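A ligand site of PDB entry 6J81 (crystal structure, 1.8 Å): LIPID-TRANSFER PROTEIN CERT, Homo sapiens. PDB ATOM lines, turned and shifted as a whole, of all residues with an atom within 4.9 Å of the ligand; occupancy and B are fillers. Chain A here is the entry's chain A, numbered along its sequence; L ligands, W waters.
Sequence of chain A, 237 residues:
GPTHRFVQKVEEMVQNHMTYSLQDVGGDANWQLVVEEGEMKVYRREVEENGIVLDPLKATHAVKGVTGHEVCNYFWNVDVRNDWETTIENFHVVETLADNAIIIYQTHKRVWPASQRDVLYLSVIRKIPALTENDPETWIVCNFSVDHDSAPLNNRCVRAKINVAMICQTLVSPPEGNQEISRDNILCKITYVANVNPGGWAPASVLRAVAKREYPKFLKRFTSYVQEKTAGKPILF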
ATOM      1  N   PHE A  75      -7.053  -7.424  18.889  1.00  0.00           N
ATOM      2  CA  PHE A  75      -5.700  -6.864  18.937  1.00  0.00           C
ATOM      3  C   PHE A  75      -4.941  -7.338  20.182  1.00  0.00           C
ATOM      4  O   PHE A  75      -3.726  -7.579  20.147  1.00  0.00           O
ATOM      5  CB  PHE A  75      -5.755  -5.319  18.807  1.00  0.00           C
ATOM      6  CG  PHE A  75      -4.393  -4.634  18.728  1.00  0.00           C
ATOM      7  CD1 PHE A  75      -3.564  -4.870  17.641  1.00  0.00           C
ATOM      8  CD2 PHE A  75      -3.937  -3.769  19.723  1.00  0.00           C
ATOM      9  CE1 PHE A  75      -2.342  -4.217  17.552  1.00  0.00           C
ATOM     10  CE2 PHE A  75      -2.681  -3.158  19.662  1.00  0.00           C
ATOM     11  CZ  PHE A  75      -1.913  -3.349  18.542  1.00  0.00           C
ATOM     12  N   ARG A  81      -3.050 -14.059  17.922  1.00  0.00           N
ATOM     13  CA  ARG A  81      -1.936 -13.225  17.475  1.00  0.00           C
ATOM     14  C   ARG A  81      -1.375 -13.757  16.155  1.00  0.00           C
ATOM     15  O   ARG A  81      -1.226 -12.997  15.199  1.00  0.00           O
ATOM     16  CB  ARG A  81      -0.947 -13.108  18.632  1.00  0.00           C
ATOM     17  CG  ARG A  81       0.228 -12.225  18.314  1.00  0.00           C
ATOM     18  CD  ARG A  81      -0.116 -10.744  18.222  1.00  0.00           C
ATOM     19  NE  ARG A  81       0.370 -10.115  19.458  1.00  0.00           N
ATOM     20  CZ  ARG A  81      -0.399  -9.625  20.420  1.00  0.00           C
ATOM     21  NH1 ARG A  81       0.180  -9.078  21.483  1.00  0.00           N
ATOM     22  NH2 ARG A  81      -1.720  -9.685  20.324  1.00  0.00           N
ATOM     23  N   TRP A  84      -2.992 -12.931  12.509  1.00  0.00           N
ATOM     24  CA  TRP A  84      -2.967 -11.701  11.736  1.00  0.00           C
ATOM     25  C   TRP A  84      -1.548 -11.118  11.674  1.00  0.00           C
ATOM     26  O   TRP A  84      -1.246 -10.380  10.737  1.00  0.00           O
ATOM     27  CB  TRP A  84      -4.014 -10.682  12.262  1.00  0.00           C
ATOM     28  CG  TRP A  84      -3.852 -10.371  13.721  1.00  0.00           C
ATOM     29  CD1 TRP A  84      -4.549 -10.903  14.773  1.00  0.00           C
ATOM     30  CD2 TRP A  84      -2.980  -9.390  14.295  1.00  0.00           C
ATOM     31  NE1 TRP A  84      -4.111 -10.365  15.975  1.00  0.00           N
ATOM     32  CE2 TRP A  84      -3.167  -9.407  15.704  1.00  0.00           C
ATOM     33  CE3 TRP A  84      -2.063  -8.478  13.747  1.00  0.00           C
ATOM     34  CZ2 TRP A  84      -2.465  -8.561  16.565  1.00  0.00           C
ATOM     35  CZ3 TRP A  84      -1.330  -7.682  14.605  1.00  0.00           C
ATOM     36  CH2 TRP A  84      -1.525  -7.731  15.996  1.00  0.00           C
ATOM     37  N   GLU A  85      -0.709 -11.439  12.657  1.00  0.00           N
ATOM     38  CA  GLU A  85       0.631 -10.856  12.713  1.00  0.00           C
ATOM     39  C   GLU A  85       1.470 -11.506  11.620  1.00  0.00           C
ATOM     40  O   GLU A  85       1.316 -12.710  11.405  1.00  0.00           O
ATOM     41  CB  GLU A  85       1.377 -11.284  13.977  1.00  0.00           C
ATOM     42  CG  GLU A  85       2.828 -10.821  13.976  1.00  0.00           C
ATOM     43  CD  GLU A  85       2.991  -9.300  14.070  1.00  0.00           C
ATOM     44  OE1 GLU A  85       2.460  -8.719  15.054  1.00  0.00           O
ATOM     45  OE2 GLU A  85       3.628  -8.706  13.184  1.00  0.00           O
ATOM     46  N   THR A  87       4.982 -10.208  11.176  1.00  0.00           N
ATOM     47  CA  THR A  87       6.364  -9.808  11.318  1.00  0.00           C
ATOM     48  C   THR A  87       7.026 -10.413  12.569  1.00  0.00           C
ATOM     49  O   THR A  87       8.183 -10.098  12.859  1.00  0.00           O
ATOM     50  CB  THR A  87       6.541  -8.280  11.294  1.00  0.00           C
ATOM     51  OG1 THR A  87       5.969  -7.779  12.492  1.00  0.00           O
ATOM     52  CG2 THR A  87       5.932  -7.619  10.064  1.00  0.00           C
ATOM     53  N   ILE A  88       6.329 -11.302  13.279  1.00  0.00           N
ATOM     54  CA  ILE A  88       6.821 -11.890  14.523  1.00  0.00           C
ATOM     55  C   ILE A  88       7.475 -13.253  14.262  1.00  0.00           C
ATOM     56  O   ILE A  88       6.891 -14.097  13.586  1.00  0.00           O
ATOM     57  CB  ILE A  88       5.615 -12.149  15.454  1.00  0.00           C
ATOM     58  CG1 ILE A  88       4.936 -10.841  15.813  1.00  0.00           C
ATOM     59  CG2 ILE A  88       6.065 -12.892  16.711  1.00  0.00           C
ATOM     60  CD1 ILE A  88       5.819  -9.982  16.607  1.00  0.00           C
ATOM     61  N   GLN A 106       8.820 -10.625  22.584  1.00  0.00           N
ATOM     62  CA  GLN A 106       8.662 -11.130  21.223  1.00  0.00           C
ATOM     63  C   GLN A 106       9.857 -10.733  20.363  1.00  0.00           C
ATOM     64  O   GLN A 106      10.541  -9.759  20.654  1.00  0.00           O
ATOM     65  CB  GLN A 106       7.352 -10.740  20.527  1.00  0.00           C
ATOM     66  CG  GLN A 106       7.291  -9.258  20.110  1.00  0.00           C
ATOM     67  CD  GLN A 106       5.924  -8.660  19.821  1.00  0.00           C
ATOM     68  OE1 GLN A 106       4.902  -9.151  20.304  1.00  0.00           O
ATOM     69  NE2 GLN A 106       5.885  -7.585  19.024  1.00  0.00           N
ATOM     70  N   HIS A 108      11.101 -10.043  16.295  1.00  0.00           N
ATOM     71  CA  HIS A 108      10.600  -9.719  14.968  1.00  0.00           C
ATOM     72  C   HIS A 108      11.492 -10.335  13.884  1.00  0.00           C
ATOM     73  O   HIS A 108      12.674 -10.490  14.086  1.00  0.00           O
ATOM     74  CB  HIS A 108      10.501  -8.181  14.837  1.00  0.00           C
ATOM     75  CG  HIS A 108       9.339  -7.647  15.602  1.00  0.00           C
ATOM     76  ND1 HIS A 108       8.077  -7.478  15.014  1.00  0.00           N
ATOM     77  CD2 HIS A 108       9.228  -7.255  16.903  1.00  0.00           C
ATOM     78  CE1 HIS A 108       7.217  -7.011  15.943  1.00  0.00           C
ATOM     79  NE2 HIS A 108       7.922  -6.876  17.126  1.00  0.00           N
ATOM     80  N   VAL A 111      14.950  -7.663   9.193  1.00  0.00           N
ATOM     81  CA  VAL A 111      14.887  -7.054   7.872  1.00  0.00           C
ATOM     82  C   VAL A 111      16.307  -6.698   7.419  1.00  0.00           C
ATOM     83  O   VAL A 111      16.933  -5.783   7.909  1.00  0.00           O
ATOM     84  CB  VAL A 111      13.921  -5.865   7.746  1.00  0.00           C
ATOM     85  CG1 VAL A 111      12.483  -6.262   8.115  1.00  0.00           C
ATOM     86  CG2 VAL A 111      14.386  -4.607   8.473  1.00  0.00           C
ATOM     87  N   ARG A 117      15.463  -7.370  15.888  1.00  0.00           N
ATOM     88  CA  ARG A 117      15.035  -6.732  17.140  1.00  0.00           C
ATOM     89  C   ARG A 117      14.147  -7.644  18.004  1.00  0.00           C
ATOM     90  O   ARG A 117      13.332  -8.426  17.486  1.00  0.00           O
ATOM     91  CB  ARG A 117      14.217  -5.474  16.808  1.00  0.00           C
ATOM     92  CG  ARG A 117      15.040  -4.191  16.893  1.00  0.00           C
ATOM     93  CD  ARG A 117      16.173  -4.163  15.854  1.00  0.00           C
ATOM     94  NE  ARG A 117      16.933  -2.932  15.938  1.00  0.00           N
ATOM     95  CZ  ARG A 117      18.051  -2.702  15.314  1.00  0.00           C
ATOM     96  NH1 ARG A 117      18.551  -3.609  14.488  1.00  0.00           N
ATOM     97  NH2 ARG A 117      18.669  -1.565  15.516  1.00  0.00           N
ATOM     98  N   TYR A 121       7.235  -5.918  26.585  1.00  0.00           N
ATOM     99  CA  TYR A 121       6.299  -4.818  26.790  1.00  0.00           C
ATOM    100  C   TYR A 121       5.103  -5.308  27.599  1.00  0.00           C
ATOM    101  O   TYR A 121       4.729  -6.491  27.532  1.00  0.00           O
ATOM    102  CB  TYR A 121       5.835  -4.247  25.421  1.00  0.00           C
ATOM    103  CG  TYR A 121       5.107  -5.202  24.513  1.00  0.00           C
ATOM    104  CD1 TYR A 121       5.855  -6.075  23.697  1.00  0.00           C
ATOM    105  CD2 TYR A 121       3.706  -5.249  24.424  1.00  0.00           C
ATOM    106  CE1 TYR A 121       5.195  -6.904  22.808  1.00  0.00           C
ATOM    107  CE2 TYR A 121       3.048  -6.083  23.526  1.00  0.00           C
ATOM    108  CZ  TYR A 121       3.826  -6.920  22.728  1.00  0.00           C
ATOM    109  OH  TYR A 121       3.256  -7.771  21.850  1.00  0.00           O
ATOM    110  N   ASN A 143       0.305  -0.908  24.416  1.00  0.00           N
ATOM    111  CA  ASN A 143       1.470  -1.792  24.519  1.00  0.00           C
ATOM    112  C   ASN A 143       2.688  -0.910  24.762  1.00  0.00           C
ATOM    113  O   ASN A 143       3.039  -0.096  23.880  1.00  0.00           O
ATOM    114  CB  ASN A 143       1.656  -2.511  23.158  1.00  0.00           C
ATOM    115  CG  ASN A 143       0.559  -3.518  22.884  1.00  0.00           C
ATOM    116  OD1 ASN A 143      -0.040  -3.995  23.835  1.00  0.00           O
ATOM    117  ND2 ASN A 143       0.248  -3.857  21.632  1.00  0.00           N
ATOM    118  N   ALA A 160      14.420  -3.273  21.083  1.00  0.00           N
ATOM    119  CA  ALA A 160      13.670  -2.072  20.732  1.00  0.00           C
ATOM    120  C   ALA A 160      12.767  -1.706  21.910  1.00  0.00           C
ATOM    121  O   ALA A 160      12.497  -2.564  22.757  1.00  0.00           O
ATOM    122  CB  ALA A 160      12.821  -2.371  19.521  1.00  0.00           C
ATOM    123  N   ILE A 162       8.955   0.335  22.751  1.00  0.00           N
ATOM    124  CA  ILE A 162       7.745   0.726  22.020  1.00  0.00           C
ATOM    125  C   ILE A 162       6.788   1.393  22.976  1.00  0.00           C
ATOM    126  O   ILE A 162       6.831   1.164  24.219  1.00  0.00           O
ATOM    127  CB  ILE A 162       7.043  -0.441  21.306  1.00  0.00           C
ATOM    128  CG1 ILE A 162       6.339  -1.407  22.279  1.00  0.00           C
ATOM    129  CG2 ILE A 162       8.001  -1.175  20.377  1.00  0.00           C
ATOM    130  CD1 ILE A 162       5.563  -2.519  21.606  1.00  0.00           C
ATOM    131  N   VAL A 164       2.748   1.961  21.967  1.00  0.00           N
ATOM    132  CA  VAL A 164       1.754   1.779  20.915  1.00  0.00           C
ATOM    133  C   VAL A 164       0.365   1.864  21.561  1.00  0.00           C
ATOM    134  O   VAL A 164       0.178   1.366  22.699  1.00  0.00           O
ATOM    135  CB  VAL A 164       1.919   0.408  20.232  1.00  0.00           C
ATOM    136  CG1 VAL A 164       0.734   0.070  19.328  1.00  0.00           C
ATOM    137  CG2 VAL A 164       3.288   0.345  19.468  1.00  0.00           C
ATOM    138  N   TYR A 192      -4.546   4.768  15.655  1.00  0.00           N
ATOM    139  CA  TYR A 192      -3.466   3.877  15.983  1.00  0.00           C
ATOM    140  C   TYR A 192      -2.200   4.707  16.042  1.00  0.00           C
ATOM    141  O   TYR A 192      -1.887   5.408  15.058  1.00  0.00           O
ATOM    142  CB  TYR A 192      -3.335   2.789  14.917  1.00  0.00           C
ATOM    143  CG  TYR A 192      -2.112   1.903  15.098  1.00  0.00           C
ATOM    144  CD1 TYR A 192      -2.094   0.832  15.971  1.00  0.00           C
ATOM    145  CD2 TYR A 192      -0.926   2.192  14.414  1.00  0.00           C
ATOM    146  CE1 TYR A 192      -0.962   0.025  16.143  1.00  0.00           C
ATOM    147  CE2 TYR A 192       0.210   1.419  14.590  1.00  0.00           C
ATOM    148  CZ  TYR A 192       0.208   0.335  15.445  1.00  0.00           C
ATOM    149  OH  TYR A 192       1.352  -0.396  15.564  1.00  0.00           O
ATOM    150  N   VAL A 196       8.343   3.962  18.180  1.00  0.00           N
ATOM    151  CA  VAL A 196       9.270   2.844  18.285  1.00  0.00           C
ATOM    152  C   VAL A 196      10.695   3.358  18.263  1.00  0.00           C
ATOM    153  O   VAL A 196      11.096   4.146  17.367  1.00  0.00           O
ATOM    154  CB  VAL A 196       9.021   1.817  17.163  1.00  0.00           C
ATOM    155  CG1 VAL A 196      10.091   0.694  17.194  1.00  0.00           C
ATOM    156  CG2 VAL A 196       7.604   1.277  17.200  1.00  0.00           C
ATOM    157  N   LEU A 207      14.711   1.424   7.894  1.00  0.00           N
ATOM    158  CA  LEU A 207      13.627   1.598   8.871  1.00  0.00           C
ATOM    159  C   LEU A 207      12.444   2.308   8.240  1.00  0.00           C
ATOM    160  O   LEU A 207      11.294   1.913   8.457  1.00  0.00           O
ATOM    161  CB  LEU A 207      14.173   2.383  10.072  1.00  0.00           C
ATOM    162  CG  LEU A 207      15.268   1.646  10.812  1.00  0.00           C
ATOM    163  CD1 LEU A 207      15.888   2.460  11.947  1.00  0.00           C
ATOM    164  CD2 LEU A 207      14.750   0.326  11.372  1.00  0.00           C
ATOM    165  N   VAL A 210      10.576  -0.022   5.785  1.00  0.00           N
ATOM    166  CA  VAL A 210       9.834  -1.029   6.546  1.00  0.00           C
ATOM    167  C   VAL A 210       8.538  -0.401   7.114  1.00  0.00           C
ATOM    168  O   VAL A 210       7.433  -0.931   6.917  1.00  0.00           O
ATOM    169  CB  VAL A 210      10.674  -1.699   7.657  1.00  0.00           C
ATOM    170  CG1 VAL A 210       9.813  -2.609   8.534  1.00  0.00           C
ATOM    171  CG2 VAL A 210      11.881  -2.481   7.119  1.00  0.00           C
ATOM    172  N   ALA A 211       8.651   0.772   7.769  1.00  0.00           N
ATOM    173  CA  ALA A 211       7.462   1.416   8.318  1.00  0.00           C
ATOM    174  C   ALA A 211       6.438   1.694   7.211  1.00  0.00           C
ATOM    175  O   ALA A 211       5.226   1.519   7.354  1.00  0.00           O
ATOM    176  CB  ALA A 211       7.838   2.687   9.063  1.00  0.00           C
ATOM    177  N   GLU A 214       4.939  -1.638   6.093  1.00  0.00           N
ATOM    178  CA  GLU A 214       4.384  -2.625   7.026  1.00  0.00           C
ATOM    179  C   GLU A 214       3.199  -2.032   7.800  1.00  0.00           C
ATOM    180  O   GLU A 214       2.338  -2.799   8.215  1.00  0.00           O
ATOM    181  CB  GLU A 214       5.426  -3.210   7.997  1.00  0.00           C
ATOM    182  CG  GLU A 214       6.459  -4.155   7.358  1.00  0.00           C
ATOM    183  CD  GLU A 214       5.954  -5.387   6.587  1.00  0.00           C
ATOM    184  OE1 GLU A 214       4.819  -5.913   6.915  1.00  0.00           O
ATOM    185  OE2 GLU A 214       6.669  -5.827   5.637  1.00  0.00           O
ATOM    186  N   TYR A 215       3.213  -0.735   8.084  1.00  0.00           N
ATOM    187  CA  TYR A 215       2.090  -0.196   8.874  1.00  0.00           C
ATOM    188  C   TYR A 215       0.759  -0.269   8.114  1.00  0.00           C
ATOM    189  O   TYR A 215      -0.285  -0.720   8.664  1.00  0.00           O
ATOM    190  CB  TYR A 215       2.385   1.204   9.432  1.00  0.00           C
ATOM    191  CG  TYR A 215       3.242   1.178  10.666  1.00  0.00           C
ATOM    192  CD1 TYR A 215       2.835   0.527  11.842  1.00  0.00           C
ATOM    193  CD2 TYR A 215       4.506   1.758  10.657  1.00  0.00           C
ATOM    194  CE1 TYR A 215       3.648   0.534  12.983  1.00  0.00           C
ATOM    195  CE2 TYR A 215       5.327   1.722  11.766  1.00  0.00           C
ATOM    196  CZ  TYR A 215       4.901   1.133  12.928  1.00  0.00           C
ATOM    197  OH  TYR A 215       5.775   1.188  14.002  1.00  0.00           O
ATOM    198  N   PHE A 218      -0.361  -3.920   7.844  1.00  0.00           N
ATOM    199  CA  PHE A 218      -0.903  -4.373   9.135  1.00  0.00           C
ATOM    200  C   PHE A 218      -2.346  -3.845   9.292  1.00  0.00           C
ATOM    201  O   PHE A 218      -3.225  -4.635   9.672  1.00  0.00           O
ATOM    202  CB  PHE A 218       0.039  -3.946  10.272  1.00  0.00           C
ATOM    203  CG  PHE A 218      -0.659  -3.657  11.587  1.00  0.00           C
ATOM    204  CD1 PHE A 218      -1.285  -4.675  12.298  1.00  0.00           C
ATOM    205  CD2 PHE A 218      -0.770  -2.364  12.043  1.00  0.00           C
ATOM    206  CE1 PHE A 218      -1.987  -4.398  13.469  1.00  0.00           C
ATOM    207  CE2 PHE A 218      -1.465  -2.076  13.220  1.00  0.00           C
ATOM    208  CZ  PHE A 218      -2.035  -3.106  13.933  1.00  0.00           C
HETATM  209  C1  LIG L   1       7.905  -1.995  14.825  1.00  0.00           C
HETATM  210  C2  LIG L   1       9.171  -1.794  14.281  1.00  0.00           C
HETATM  211  C3  LIG L   1      10.301  -2.400  14.916  1.00  0.00           C
HETATM  212  C4  LIG L   1       7.728  -2.828  15.969  1.00  0.00           C
HETATM  213  C5  LIG L   1       6.151  -3.539  17.805  1.00  0.00           C
HETATM  214  C6  LIG L   1       6.372  -3.029  16.491  1.00  0.00           C
HETATM  215  C7  LIG L   1       8.857  -3.402  16.586  1.00  0.00           C
HETATM  216  C8  LIG L   1       3.941  -2.894  16.099  1.00  0.00           C
HETATM  217  C9  LIG L   1       4.812  -3.726  18.240  1.00  0.00           C
HETATM  218  O1  LIG L   1       1.224  -2.799  17.093  1.00  0.00           O
HETATM  219  S1  LIG L   1       2.089  -3.569  17.998  1.00  0.00           S
HETATM  220  O2  LIG L   1       2.270  -3.426  19.440  1.00  0.00           O
HETATM  221  C10 LIG L   1       1.439  -5.259  17.655  1.00  0.00           C
HETATM  222  C11 LIG L   1       2.155  -6.307  18.561  1.00  0.00           C
HETATM  223  O3  LIG L   1       3.344  -6.710  17.853  1.00  0.00           O
HETATM  224  C12 LIG L   1       3.773  -3.370  17.422  1.00  0.00           C
HETATM  225  C13 LIG L   1       5.270  -2.730  15.663  1.00  0.00           C
HETATM  226  C14 LIG L   1      11.664  -2.144  14.271  1.00  0.00           C
HETATM  227  C15 LIG L   1      12.254  -3.465  13.712  1.00  0.00           C
HETATM  228  C16 LIG L   1      13.628  -3.321  13.062  1.00  0.00           C
HETATM  229  C17 LIG L   1      10.177  -3.225  16.049  1.00  0.00           C
HETATM  230  C18 LIG L   1       9.320  -0.891  13.060  1.00  0.00           C
HETATM  231  C19 LIG L   1       9.929  -1.418  11.800  1.00  0.00           C
HETATM  232  C20 LIG L   1       8.444  -1.048  11.812  1.00  0.00           C
HETATM  233  C21 LIG L   1       7.404  -2.147  11.724  1.00  0.00           C
HETATM  234  N1  LIG L   1       7.928  -3.435  11.867  1.00  0.00           N
HETATM  235  C22 LIG L   1       7.059  -4.485  11.863  1.00  0.00           C
HETATM  236  C23 LIG L   1       5.642  -4.311  11.693  1.00  0.00           C
HETATM  237  C24 LIG L   1       5.103  -3.011  11.519  1.00  0.00           C
HETATM  238  C25 LIG L   1       6.001  -1.921  11.549  1.00  0.00           C
HETATM  239  O   HOH W   1       3.552  -6.380  15.185  1.00  0.00           O
HETATM  240  O   HOH W   2      10.394  -5.196  11.763  1.00  0.00           O
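ND2 of Asn 143 is in hydrogen-bond range of O2 of the ligand, at 3.0 Å. The side-chain hydroxyl of Tyr 192 is in hydrogen-bond range of an oxygen (O1) of the ligand, 2.9 Å away. The side-chain amide nitrogen (NE2) of Gln 106 sits at hydrogen-bond distance from an oxygen (O3) of the ligand (2.9 Å).
The side-chain hydroxyl (OG1) of Thr 87 is in hydrogen-bond range of a ring nitrogen (ND1) of His 108, 3.3 Å away. The backbone carbonyl oxygen of Asn 143 is in hydrogen-bond range of the backbone NH of Val 164, at 2.8 Å. The guanidinium group (NH2) of Arg 81 lies within hydrogen-bond range of the backbone carbonyl oxygen (O) of Phe 75, at 2.9 Å. OE2 of Glu 85 lies within hydrogen-bond range of OG1 of Thr 87, 2.6 Å away. The backbone NH of His 108 is in hydrogen-bond range of the backbone carbonyl oxygen of Arg 117 (3.0 Å). The side-chain amide nitrogen of Gln 106 sits at hydrogen-bond distance from a ring nitrogen (NE2) of His 108, at 2.9 Å. The side-chain amide oxygen of Gln 106 sits at hydrogen-bond distance from the side-chain hydroxyl of Tyr 121, 2.6 Å away. NH1 of Arg 81 is in hydrogen-bond range of OH of Tyr 121, at 3.4 Å.
Residues that only touch the ligand: Val 210 (3.5 Å), Phe 75 (3.5 Å), Thr 87 (3.5 Å), Tyr 215 (3.5 Å), Glu 214 (3.5 Å), Glu 85 (3.6 Å), His 108 (3.6 Å), Ile 162 (3.7 Å), Val 164 (3.7 Å), Tyr 121 (3.8 Å), Val 196 (3.8 Å) and Arg 117 (3.9 Å). Within 4 Å of the ligand: Phe 75, Glu 85, Thr 87, Gln 106, His 108, Arg 117, Tyr 121, Asn 143, Ile 162, Val 164, Tyr 192, Val 196, Val 210, Glu 214 and Tyr 215.
Water W1 bridges the side-chain carboxylate (OE1) of Glu 85 (2.6 Å) and an oxygen (O3) of the ligand (2.7 Å).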
